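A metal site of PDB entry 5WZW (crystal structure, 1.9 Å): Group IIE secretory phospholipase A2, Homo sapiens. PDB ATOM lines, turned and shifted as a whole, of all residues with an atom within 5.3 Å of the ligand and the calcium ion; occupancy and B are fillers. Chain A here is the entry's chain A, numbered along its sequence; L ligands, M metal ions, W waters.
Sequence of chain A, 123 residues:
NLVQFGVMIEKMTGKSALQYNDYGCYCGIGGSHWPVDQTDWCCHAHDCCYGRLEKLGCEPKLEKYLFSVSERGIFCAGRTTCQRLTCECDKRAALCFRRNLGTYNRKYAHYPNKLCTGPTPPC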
ATOM      1  N   LEU A   2      14.687 -10.810 -11.365  1.00  0.00           N
ATOM      2  CA  LEU A   2      14.028 -10.856 -10.076  1.00  0.00           C
ATOM      3  C   LEU A   2      13.716  -9.436  -9.604  1.00  0.00           C
ATOM      4  O   LEU A   2      12.952  -9.267  -8.671  1.00  0.00           O
ATOM      5  CB  LEU A   2      14.876 -11.613  -9.046  1.00  0.00           C
ATOM      6  CG  LEU A   2      14.834 -13.157  -9.051  1.00  0.00           C
ATOM      7  CD1 LEU A   2      14.363 -13.783 -10.365  1.00  0.00           C
ATOM      8  CD2 LEU A   2      16.199 -13.704  -8.644  1.00  0.00           C
ATOM      9  N   VAL A   3      14.304  -8.434 -10.263  1.00  0.00           N
ATOM     10  CA  VAL A   3      13.802  -7.046 -10.145  1.00  0.00           C
ATOM     11  C   VAL A   3      12.341  -7.056 -10.604  1.00  0.00           C
ATOM     12  O   VAL A   3      11.458  -6.639  -9.856  1.00  0.00           O
ATOM     13  CB  VAL A   3      14.584  -6.000 -10.978  1.00  0.00           C
ATOM     14  CG1 VAL A   3      14.252  -4.594 -10.474  1.00  0.00           C
ATOM     15  CG2 VAL A   3      16.103  -6.250 -10.913  1.00  0.00           C
ATOM     16  N   PHE A   5      10.203  -9.844 -11.264  1.00  0.00           N
ATOM     17  CA  PHE A   5       9.333 -10.743 -10.457  1.00  0.00           C
ATOM     18  C   PHE A   5       9.078 -10.145  -9.083  1.00  0.00           C
ATOM     19  O   PHE A   5       7.942 -10.074  -8.620  1.00  0.00           O
ATOM     20  CB  PHE A   5       9.933 -12.151 -10.334  1.00  0.00           C
ATOM     21  CG  PHE A   5       9.009 -13.164  -9.648  1.00  0.00           C
ATOM     22  CD1 PHE A   5       7.609 -13.094  -9.748  1.00  0.00           C
ATOM     23  CD2 PHE A   5       9.558 -14.202  -8.916  1.00  0.00           C
ATOM     24  CE1 PHE A   5       6.802 -14.038  -9.118  1.00  0.00           C
ATOM     25  CE2 PHE A   5       8.753 -15.145  -8.300  1.00  0.00           C
ATOM     26  CZ  PHE A   5       7.367 -15.062  -8.391  1.00  0.00           C
ATOM     27  N   GLY A   6      10.149  -9.658  -8.460  1.00  0.00           N
ATOM     28  CA  GLY A   6      10.047  -8.938  -7.194  1.00  0.00           C
ATOM     29  C   GLY A   6       9.091  -7.764  -7.223  1.00  0.00           C
ATOM     30  O   GLY A   6       8.252  -7.612  -6.328  1.00  0.00           O
ATOM     31  N   ILE A   9       5.611  -9.152  -7.406  1.00  0.00           N
ATOM     32  CA  ILE A   9       5.169  -9.647  -6.098  1.00  0.00           C
ATOM     33  C   ILE A   9       4.685  -8.504  -5.208  1.00  0.00           C
ATOM     34  O   ILE A   9       3.610  -8.589  -4.595  1.00  0.00           O
ATOM     35  CB  ILE A   9       6.265 -10.433  -5.371  1.00  0.00           C
ATOM     36  CG1 ILE A   9       6.538 -11.758  -6.111  1.00  0.00           C
ATOM     37  CG2 ILE A   9       5.863 -10.729  -3.920  1.00  0.00           C
ATOM     38  CD1 ILE A   9       7.909 -12.313  -5.831  1.00  0.00           C
ATOM     39  N   ALA A  17       9.165  -8.140  -1.629  1.00  0.00           N
ATOM     40  CA  ALA A  17       9.562  -9.365  -2.331  1.00  0.00           C
ATOM     41  C   ALA A  17      10.402 -10.305  -1.446  1.00  0.00           C
ATOM     42  O   ALA A  17      10.345 -11.532  -1.595  1.00  0.00           O
ATOM     43  CB  ALA A  17      10.316  -9.021  -3.606  1.00  0.00           C
ATOM     44  N   LEU A  18      11.157  -9.713  -0.515  1.00  0.00           N
ATOM     45  CA  LEU A  18      11.996 -10.476   0.406  1.00  0.00           C
ATOM     46  C   LEU A  18      11.196 -11.316   1.423  1.00  0.00           C
ATOM     47  O   LEU A  18      11.759 -12.222   2.029  1.00  0.00           O
ATOM     48  CB  LEU A  18      12.955  -9.539   1.144  1.00  0.00           C
ATOM     49  CG  LEU A  18      13.859  -8.658   0.277  1.00  0.00           C
ATOM     50  CD1 LEU A  18      14.735  -7.778   1.160  1.00  0.00           C
ATOM     51  CD2 LEU A  18      14.699  -9.508  -0.664  1.00  0.00           C
ATOM     52  N   TYR A  20       8.786 -13.204   0.438  1.00  0.00           N
ATOM     53  CA  TYR A  20       8.536 -14.449  -0.265  1.00  0.00           C
ATOM     54  C   TYR A  20       9.823 -15.269  -0.504  1.00  0.00           C
ATOM     55  O   TYR A  20       9.739 -16.494  -0.535  1.00  0.00           O
ATOM     56  CB  TYR A  20       7.722 -14.196  -1.527  1.00  0.00           C
ATOM     57  CG  TYR A  20       6.276 -13.894  -1.212  1.00  0.00           C
ATOM     58  CD1 TYR A  20       5.335 -14.918  -1.092  1.00  0.00           C
ATOM     59  CD2 TYR A  20       5.842 -12.579  -0.971  1.00  0.00           C
ATOM     60  CE1 TYR A  20       4.017 -14.663  -0.781  1.00  0.00           C
ATOM     61  CE2 TYR A  20       4.511 -12.309  -0.662  1.00  0.00           C
ATOM     62  CZ  TYR A  20       3.598 -13.351  -0.560  1.00  0.00           C
ATOM     63  OH  TYR A  20       2.289 -13.103  -0.262  1.00  0.00           O
ATOM     64  N   ASN A  21      10.986 -14.635  -0.603  1.00  0.00           N
ATOM     65  CA  ASN A  21      12.253 -15.377  -0.581  1.00  0.00           C
ATOM     66  C   ASN A  21      12.444 -16.214   0.696  1.00  0.00           C
ATOM     67  O   ASN A  21      12.236 -15.737   1.819  1.00  0.00           O
ATOM     68  CB  ASN A  21      13.454 -14.436  -0.731  1.00  0.00           C
ATOM     69  CG  ASN A  21      14.794 -15.174  -0.777  1.00  0.00           C
ATOM     70  OD1 ASN A  21      15.780 -14.737  -0.180  1.00  0.00           O
ATOM     71  ND2 ASN A  21      14.812 -16.304  -1.479  1.00  0.00           N
ATOM     72  N   TYR A  26       9.850 -24.203  -0.669  1.00  0.00           N
ATOM     73  CA  TYR A  26      10.016 -23.966  -2.108  1.00  0.00           C
ATOM     74  C   TYR A  26      10.270 -22.526  -2.560  1.00  0.00           C
ATOM     75  O   TYR A  26      10.811 -22.359  -3.636  1.00  0.00           O
ATOM     76  CB  TYR A  26       8.831 -24.557  -2.889  1.00  0.00           C
ATOM     77  CG  TYR A  26       8.933 -26.045  -2.918  1.00  0.00           C
ATOM     78  CD1 TYR A  26       9.668 -26.686  -3.900  1.00  0.00           C
ATOM     79  CD2 TYR A  26       8.371 -26.810  -1.898  1.00  0.00           C
ATOM     80  CE1 TYR A  26       9.808 -28.059  -3.916  1.00  0.00           C
ATOM     81  CE2 TYR A  26       8.510 -28.183  -1.900  1.00  0.00           C
ATOM     82  CZ  TYR A  26       9.228 -28.802  -2.913  1.00  0.00           C
ATOM     83  OH  TYR A  26       9.362 -30.167  -2.930  1.00  0.00           O
ATOM     84  N   CYS A  27       9.876 -21.518  -1.795  1.00  0.00           N
ATOM     85  CA  CYS A  27      10.114 -20.133  -2.256  1.00  0.00           C
ATOM     86  C   CYS A  27      11.580 -19.747  -2.052  1.00  0.00           C
ATOM     87  O   CYS A  27      12.089 -19.722  -0.929  1.00  0.00           O
ATOM     88  CB  CYS A  27       9.204 -19.157  -1.545  1.00  0.00           C
ATOM     89  SG  CYS A  27       7.457 -19.577  -1.637  1.00  0.00           S
ATOM     90  N   GLY A  28      12.252 -19.414  -3.146  1.00  0.00           N
ATOM     91  CA  GLY A  28      13.707 -19.208  -3.151  1.00  0.00           C
ATOM     92  C   GLY A  28      14.325 -20.202  -4.115  1.00  0.00           C
ATOM     93  O   GLY A  28      13.598 -20.940  -4.779  1.00  0.00           O
ATOM     94  N   ILE A  29      15.646 -20.216  -4.210  1.00  0.00           N
ATOM     95  CA  ILE A  29      16.298 -21.112  -5.162  1.00  0.00           C
ATOM     96  C   ILE A  29      16.196 -22.576  -4.690  1.00  0.00           C
ATOM     97  O   ILE A  29      16.487 -22.887  -3.540  1.00  0.00           O
ATOM     98  CB  ILE A  29      17.780 -20.696  -5.413  1.00  0.00           C
ATOM     99  CG1 ILE A  29      17.825 -19.301  -6.057  1.00  0.00           C
ATOM    100  CG2 ILE A  29      18.481 -21.717  -6.316  1.00  0.00           C
ATOM    101  CD1 ILE A  29      19.202 -18.639  -6.034  1.00  0.00           C
ATOM    102  N   GLY A  30      15.755 -23.450  -5.587  1.00  0.00           N
ATOM    103  CA  GLY A  30      15.647 -24.888  -5.309  1.00  0.00           C
ATOM    104  C   GLY A  30      14.428 -25.220  -4.466  1.00  0.00           C
ATOM    105  O   GLY A  30      13.439 -24.485  -4.459  1.00  0.00           O
ATOM    106  N   GLY A  31      14.502 -26.331  -3.762  1.00  0.00           N
ATOM    107  CA  GLY A  31      13.427 -26.763  -2.901  1.00  0.00           C
ATOM    108  C   GLY A  31      13.245 -28.261  -2.947  1.00  0.00           C
ATOM    109  O   GLY A  31      13.536 -28.893  -3.945  1.00  0.00           O
ATOM    110  N   CYS A  42       2.494 -22.414  -4.350  1.00  0.00           N
ATOM    111  CA  CYS A  42       2.668 -21.466  -5.471  1.00  0.00           C
ATOM    112  C   CYS A  42       4.106 -21.529  -5.965  1.00  0.00           C
ATOM    113  O   CYS A  42       4.343 -21.524  -7.174  1.00  0.00           O
ATOM    114  CB  CYS A  42       2.368 -20.016  -5.062  1.00  0.00           C
ATOM    115  SG  CYS A  42       0.734 -19.677  -4.379  1.00  0.00           S
ATOM    116  N   CYS A  43       5.056 -21.606  -5.026  1.00  0.00           N
ATOM    117  CA  CYS A  43       6.478 -21.678  -5.350  1.00  0.00           C
ATOM    118  C   CYS A  43       6.894 -22.998  -5.979  1.00  0.00           C
ATOM    119  O   CYS A  43       7.667 -23.014  -6.932  1.00  0.00           O
ATOM    120  CB  CYS A  43       7.333 -21.351  -4.122  1.00  0.00           C
ATOM    121  SG  CYS A  43       7.107 -19.626  -3.624  1.00  0.00           S
ATOM    122  N   HIS A  44       6.387 -24.103  -5.445  1.00  0.00           N
ATOM    123  CA  HIS A  44       6.572 -25.411  -6.068  1.00  0.00           C
ATOM    124  C   HIS A  44       6.165 -25.359  -7.542  1.00  0.00           C
ATOM    125  O   HIS A  44       6.928 -25.749  -8.419  1.00  0.00           O
ATOM    126  CB  HIS A  44       5.767 -26.472  -5.317  1.00  0.00           C
ATOM    127  CG  HIS A  44       5.858 -27.836  -5.932  1.00  0.00           C
ATOM    128  ND1 HIS A  44       4.972 -28.278  -6.879  1.00  0.00           N
ATOM    129  CD2 HIS A  44       6.756 -28.830  -5.745  1.00  0.00           C
ATOM    130  CE1 HIS A  44       5.295 -29.503  -7.241  1.00  0.00           C
ATOM    131  NE2 HIS A  44       6.375 -29.868  -6.564  1.00  0.00           N
ATOM    132  N   HIS A  46       5.736 -22.673  -9.512  1.00  0.00           N
ATOM    133  CA  HIS A  46       6.593 -21.721 -10.215  1.00  0.00           C
ATOM    134  C   HIS A  46       7.946 -22.355 -10.615  1.00  0.00           C
ATOM    135  O   HIS A  46       8.407 -22.156 -11.730  1.00  0.00           O
ATOM    136  CB  HIS A  46       6.785 -20.493  -9.327  1.00  0.00           C
ATOM    137  CG  HIS A  46       7.535 -19.375  -9.979  1.00  0.00           C
ATOM    138  ND1 HIS A  46       8.849 -19.099  -9.689  1.00  0.00           N
ATOM    139  CD2 HIS A  46       7.149 -18.469 -10.903  1.00  0.00           C
ATOM    140  CE1 HIS A  46       9.249 -18.069 -10.416  1.00  0.00           C
ATOM    141  NE2 HIS A  46       8.231 -17.669 -11.148  1.00  0.00           N
ATOM    142  N   ASP A  47       8.553 -23.151  -9.725  1.00  0.00           N
ATOM    143  CA  ASP A  47       9.746 -23.946 -10.069  1.00  0.00           C
ATOM    144  C   ASP A  47       9.472 -24.890 -11.237  1.00  0.00           C
ATOM    145  O   ASP A  47      10.284 -24.976 -12.157  1.00  0.00           O
ATOM    146  CB  ASP A  47      10.214 -24.762  -8.869  1.00  0.00           C
ATOM    147  CG  ASP A  47      10.843 -23.928  -7.769  1.00  0.00           C
ATOM    148  OD1 ASP A  47      11.039 -22.693  -7.923  1.00  0.00           O
ATOM    149  OD2 ASP A  47      11.146 -24.505  -6.711  1.00  0.00           O
ATOM    150  N   TYR A  50       9.227 -22.804 -14.399  1.00  0.00           N
ATOM    151  CA  TYR A  50      10.576 -22.520 -14.910  1.00  0.00           C
ATOM    152  C   TYR A  50      11.236 -23.736 -15.570  1.00  0.00           C
ATOM    153  O   TYR A  50      11.892 -23.598 -16.602  1.00  0.00           O
ATOM    154  CB  TYR A  50      11.467 -21.900 -13.840  1.00  0.00           C
ATOM    155  CG  TYR A  50      11.337 -20.381 -13.672  1.00  0.00           C
ATOM    156  CD1 TYR A  50      10.189 -19.666 -14.043  1.00  0.00           C
ATOM    157  CD2 TYR A  50      12.370 -19.664 -13.089  1.00  0.00           C
ATOM    158  CE1 TYR A  50      10.088 -18.291 -13.843  1.00  0.00           C
ATOM    159  CE2 TYR A  50      12.299 -18.290 -12.893  1.00  0.00           C
ATOM    160  CZ  TYR A  50      11.154 -17.600 -13.263  1.00  0.00           C
ATOM    161  OH  TYR A  50      11.143 -16.223 -13.037  1.00  0.00           O
ATOM    162  N   LYS A  61      15.535 -17.936 -15.393  1.00  0.00           N
ATOM    163  CA  LYS A  61      16.242 -17.262 -14.304  1.00  0.00           C
ATOM    164  C   LYS A  61      16.897 -15.976 -14.732  1.00  0.00           C
ATOM    165  O   LYS A  61      17.136 -15.124 -13.890  1.00  0.00           O
ATOM    166  CB  LYS A  61      17.311 -18.163 -13.674  1.00  0.00           C
ATOM    167  CG  LYS A  61      16.733 -19.376 -12.957  1.00  0.00           C
ATOM    168  CD  LYS A  61      17.822 -20.279 -12.389  1.00  0.00           C
ATOM    169  CE  LYS A  61      17.477 -21.747 -12.555  1.00  0.00           C
ATOM    170  NZ  LYS A  61      18.248 -22.624 -11.644  1.00  0.00           N
ATOM    171  N   PHE A  97       0.137 -16.068  -5.013  1.00  0.00           N
ATOM    172  CA  PHE A  97       0.495 -15.414  -3.756  1.00  0.00           C
ATOM    173  C   PHE A  97      -0.654 -14.547  -3.235  1.00  0.00           C
ATOM    174  O   PHE A  97      -1.040 -14.688  -2.067  1.00  0.00           O
ATOM    175  CB  PHE A  97       1.759 -14.547  -3.884  1.00  0.00           C
ATOM    176  CG  PHE A  97       3.035 -15.311  -4.125  1.00  0.00           C
ATOM    177  CD1 PHE A  97       3.192 -16.671  -3.796  1.00  0.00           C
ATOM    178  CD2 PHE A  97       4.144 -14.638  -4.645  1.00  0.00           C
ATOM    179  CE1 PHE A  97       4.393 -17.311  -4.017  1.00  0.00           C
ATOM    180  CE2 PHE A  97       5.347 -15.274  -4.844  1.00  0.00           C
ATOM    181  CZ  PHE A  97       5.465 -16.617  -4.542  1.00  0.00           C
HETATM  182  N1  LIG L   1      12.238 -15.907  -5.079  1.00  0.00           N
HETATM  183  C1  LIG L   1      11.041 -16.488  -5.070  1.00  0.00           C
HETATM  184  C2  LIG L   1      11.005 -17.401  -6.027  1.00  0.00           C
HETATM  185  C3  LIG L   1      12.178 -17.404  -6.656  1.00  0.00           C
HETATM  186  C4  LIG L   1      12.636 -18.132  -7.690  1.00  0.00           C
HETATM  187  C5  LIG L   1      13.935 -17.956  -8.173  1.00  0.00           C
HETATM  188  C6  LIG L   1      14.738 -16.996  -7.555  1.00  0.00           C
HETATM  189  C7  LIG L   1      14.210 -16.259  -6.488  1.00  0.00           C
HETATM  190  C8  LIG L   1      12.952 -16.472  -6.057  1.00  0.00           C
HETATM  191  C9  LIG L   1       9.886 -16.181  -4.131  1.00  0.00           C
HETATM  192  C10 LIG L   1       9.803 -18.306  -6.377  1.00  0.00           C
HETATM  193  O1  LIG L   1      14.404 -18.704  -9.227  1.00  0.00           O
HETATM  194  C11 LIG L   1      12.741 -14.846  -4.187  1.00  0.00           C
HETATM  195  C12 LIG L   1      12.917 -10.993  -5.944  1.00  0.00           C
HETATM  196  C13 LIG L   1      13.590 -11.286  -4.772  1.00  0.00           C
HETATM  197  C14 LIG L   1      13.509 -12.563  -4.217  1.00  0.00           C
HETATM  198  C15 LIG L   1      12.754 -13.574  -4.843  1.00  0.00           C
HETATM  199  C16 LIG L   1      12.070 -13.266  -6.031  1.00  0.00           C
HETATM  200  C17 LIG L   1      12.168 -11.988  -6.583  1.00  0.00           C
HETATM  201  C18 LIG L   1       8.925 -15.340  -4.954  1.00  0.00           C
HETATM  202  C19 LIG L   1      10.163 -19.780  -6.157  1.00  0.00           C
HETATM  203  O2  LIG L   1      11.152 -20.111  -5.528  1.00  0.00           O
HETATM  204  N2  LIG L   1       9.338 -20.630  -6.699  1.00  0.00           N
HETATM  205  C20 LIG L   1      14.608 -20.108  -8.949  1.00  0.00           C
HETATM  206  C21 LIG L   1      14.950 -20.745 -10.283  1.00  0.00           C
HETATM  207  P1  LIG L   1      15.065 -23.325  -9.081  1.00  0.00           P
HETATM  208  O3  LIG L   1      14.661 -24.546  -9.789  1.00  0.00           O
HETATM  209  O4  LIG L   1      16.476 -22.910  -9.148  1.00  0.00           O
HETATM  210  O5  LIG L   1      14.278 -22.934  -7.893  1.00  0.00           O
HETATM  211  C22 LIG L   1      14.320 -22.140 -10.309  1.00  0.00           C
HETATM  212 CA    CA M   1      12.204 -22.706  -5.357  1.00  0.00          CA
HETATM  213  O   HOH W   1      12.855 -25.045 -11.922  1.00  0.00           O
HETATM  214  O   HOH W   2      10.978 -20.840  -9.727  1.00  0.00           O
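The backbone NH of Gly 28 sits close to an oxygen (O2) of the ligand (2.7 Å).
N of Gly 30 is in hydrogen-bond range of O5 of the ligand, at 2.8 Å.
The backbone carbonyl oxygen (O) of Cys 43 is in hydrogen-bond range of a nitrogen (N2) of the ligand.
An oxygen (O4) of the ligand lies within salt-bridge range of the side-chain amino group (NZ) of Lys 61 (3.1 Å).
ND1 of His 46 lies within hydrogen-bond range of N2 of the ligand.
The side-chain sulfur of Cys 43 is disulfide-bonded to the side-chain sulfur of Cys 27 (2.0 Å).
SG of Cys 42 lies within hydrogen-bond range of N of Phe 97, at 3.7 Å.
Residues that only touch the ligand: Leu 2 (3.2 Å), Ile 9 (3.3 Å), Phe 5 (3.4 Å), Cys 27 (3.4 Å), Asn 21 (3.6 Å), Phe 97 (3.6 Å), Gly 6 (3.6 Å), Tyr 20 (3.6 Å), Ile 29 (3.7 Å) and Tyr 50 (3.96 Å).
Hydrophobic or aromatic side chains that line the ligand: Leu 2, Phe 5, Ile 9, Tyr 20, Ile 29, His 46, Tyr 50 and Phe 97.
Of the 23 residues printed, 17 come within 4 Å of the ligand.
The calcium ion is bound by the backbone carbonyl oxygen (O) of Tyr 26 (2.2 Å), the backbone carbonyl oxygen (O) of Gly 28 (2.3 Å), the backbone carbonyl oxygen (O) of Gly 30 (2.3 Å), the side-chain carboxylate (OD2) of Asp 47 (2.5 Å), an oxygen (O2) of the ligand (2.8 Å) and the side-chain carboxylate (OD1) of Asp 47 (2.8 Å).
The calcium ion has six donor atoms within binding distance.
Water W1 bridges O of Asp 47 and O3 of the ligand.
Water W2 lies within hydrogen-bond range of a ring nitrogen (ND1) of His 46 (2.8 Å), the backbone NH (N) of Asp 47 (3.3 Å) and a nitrogen (N2) of the ligand (3.4 Å).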
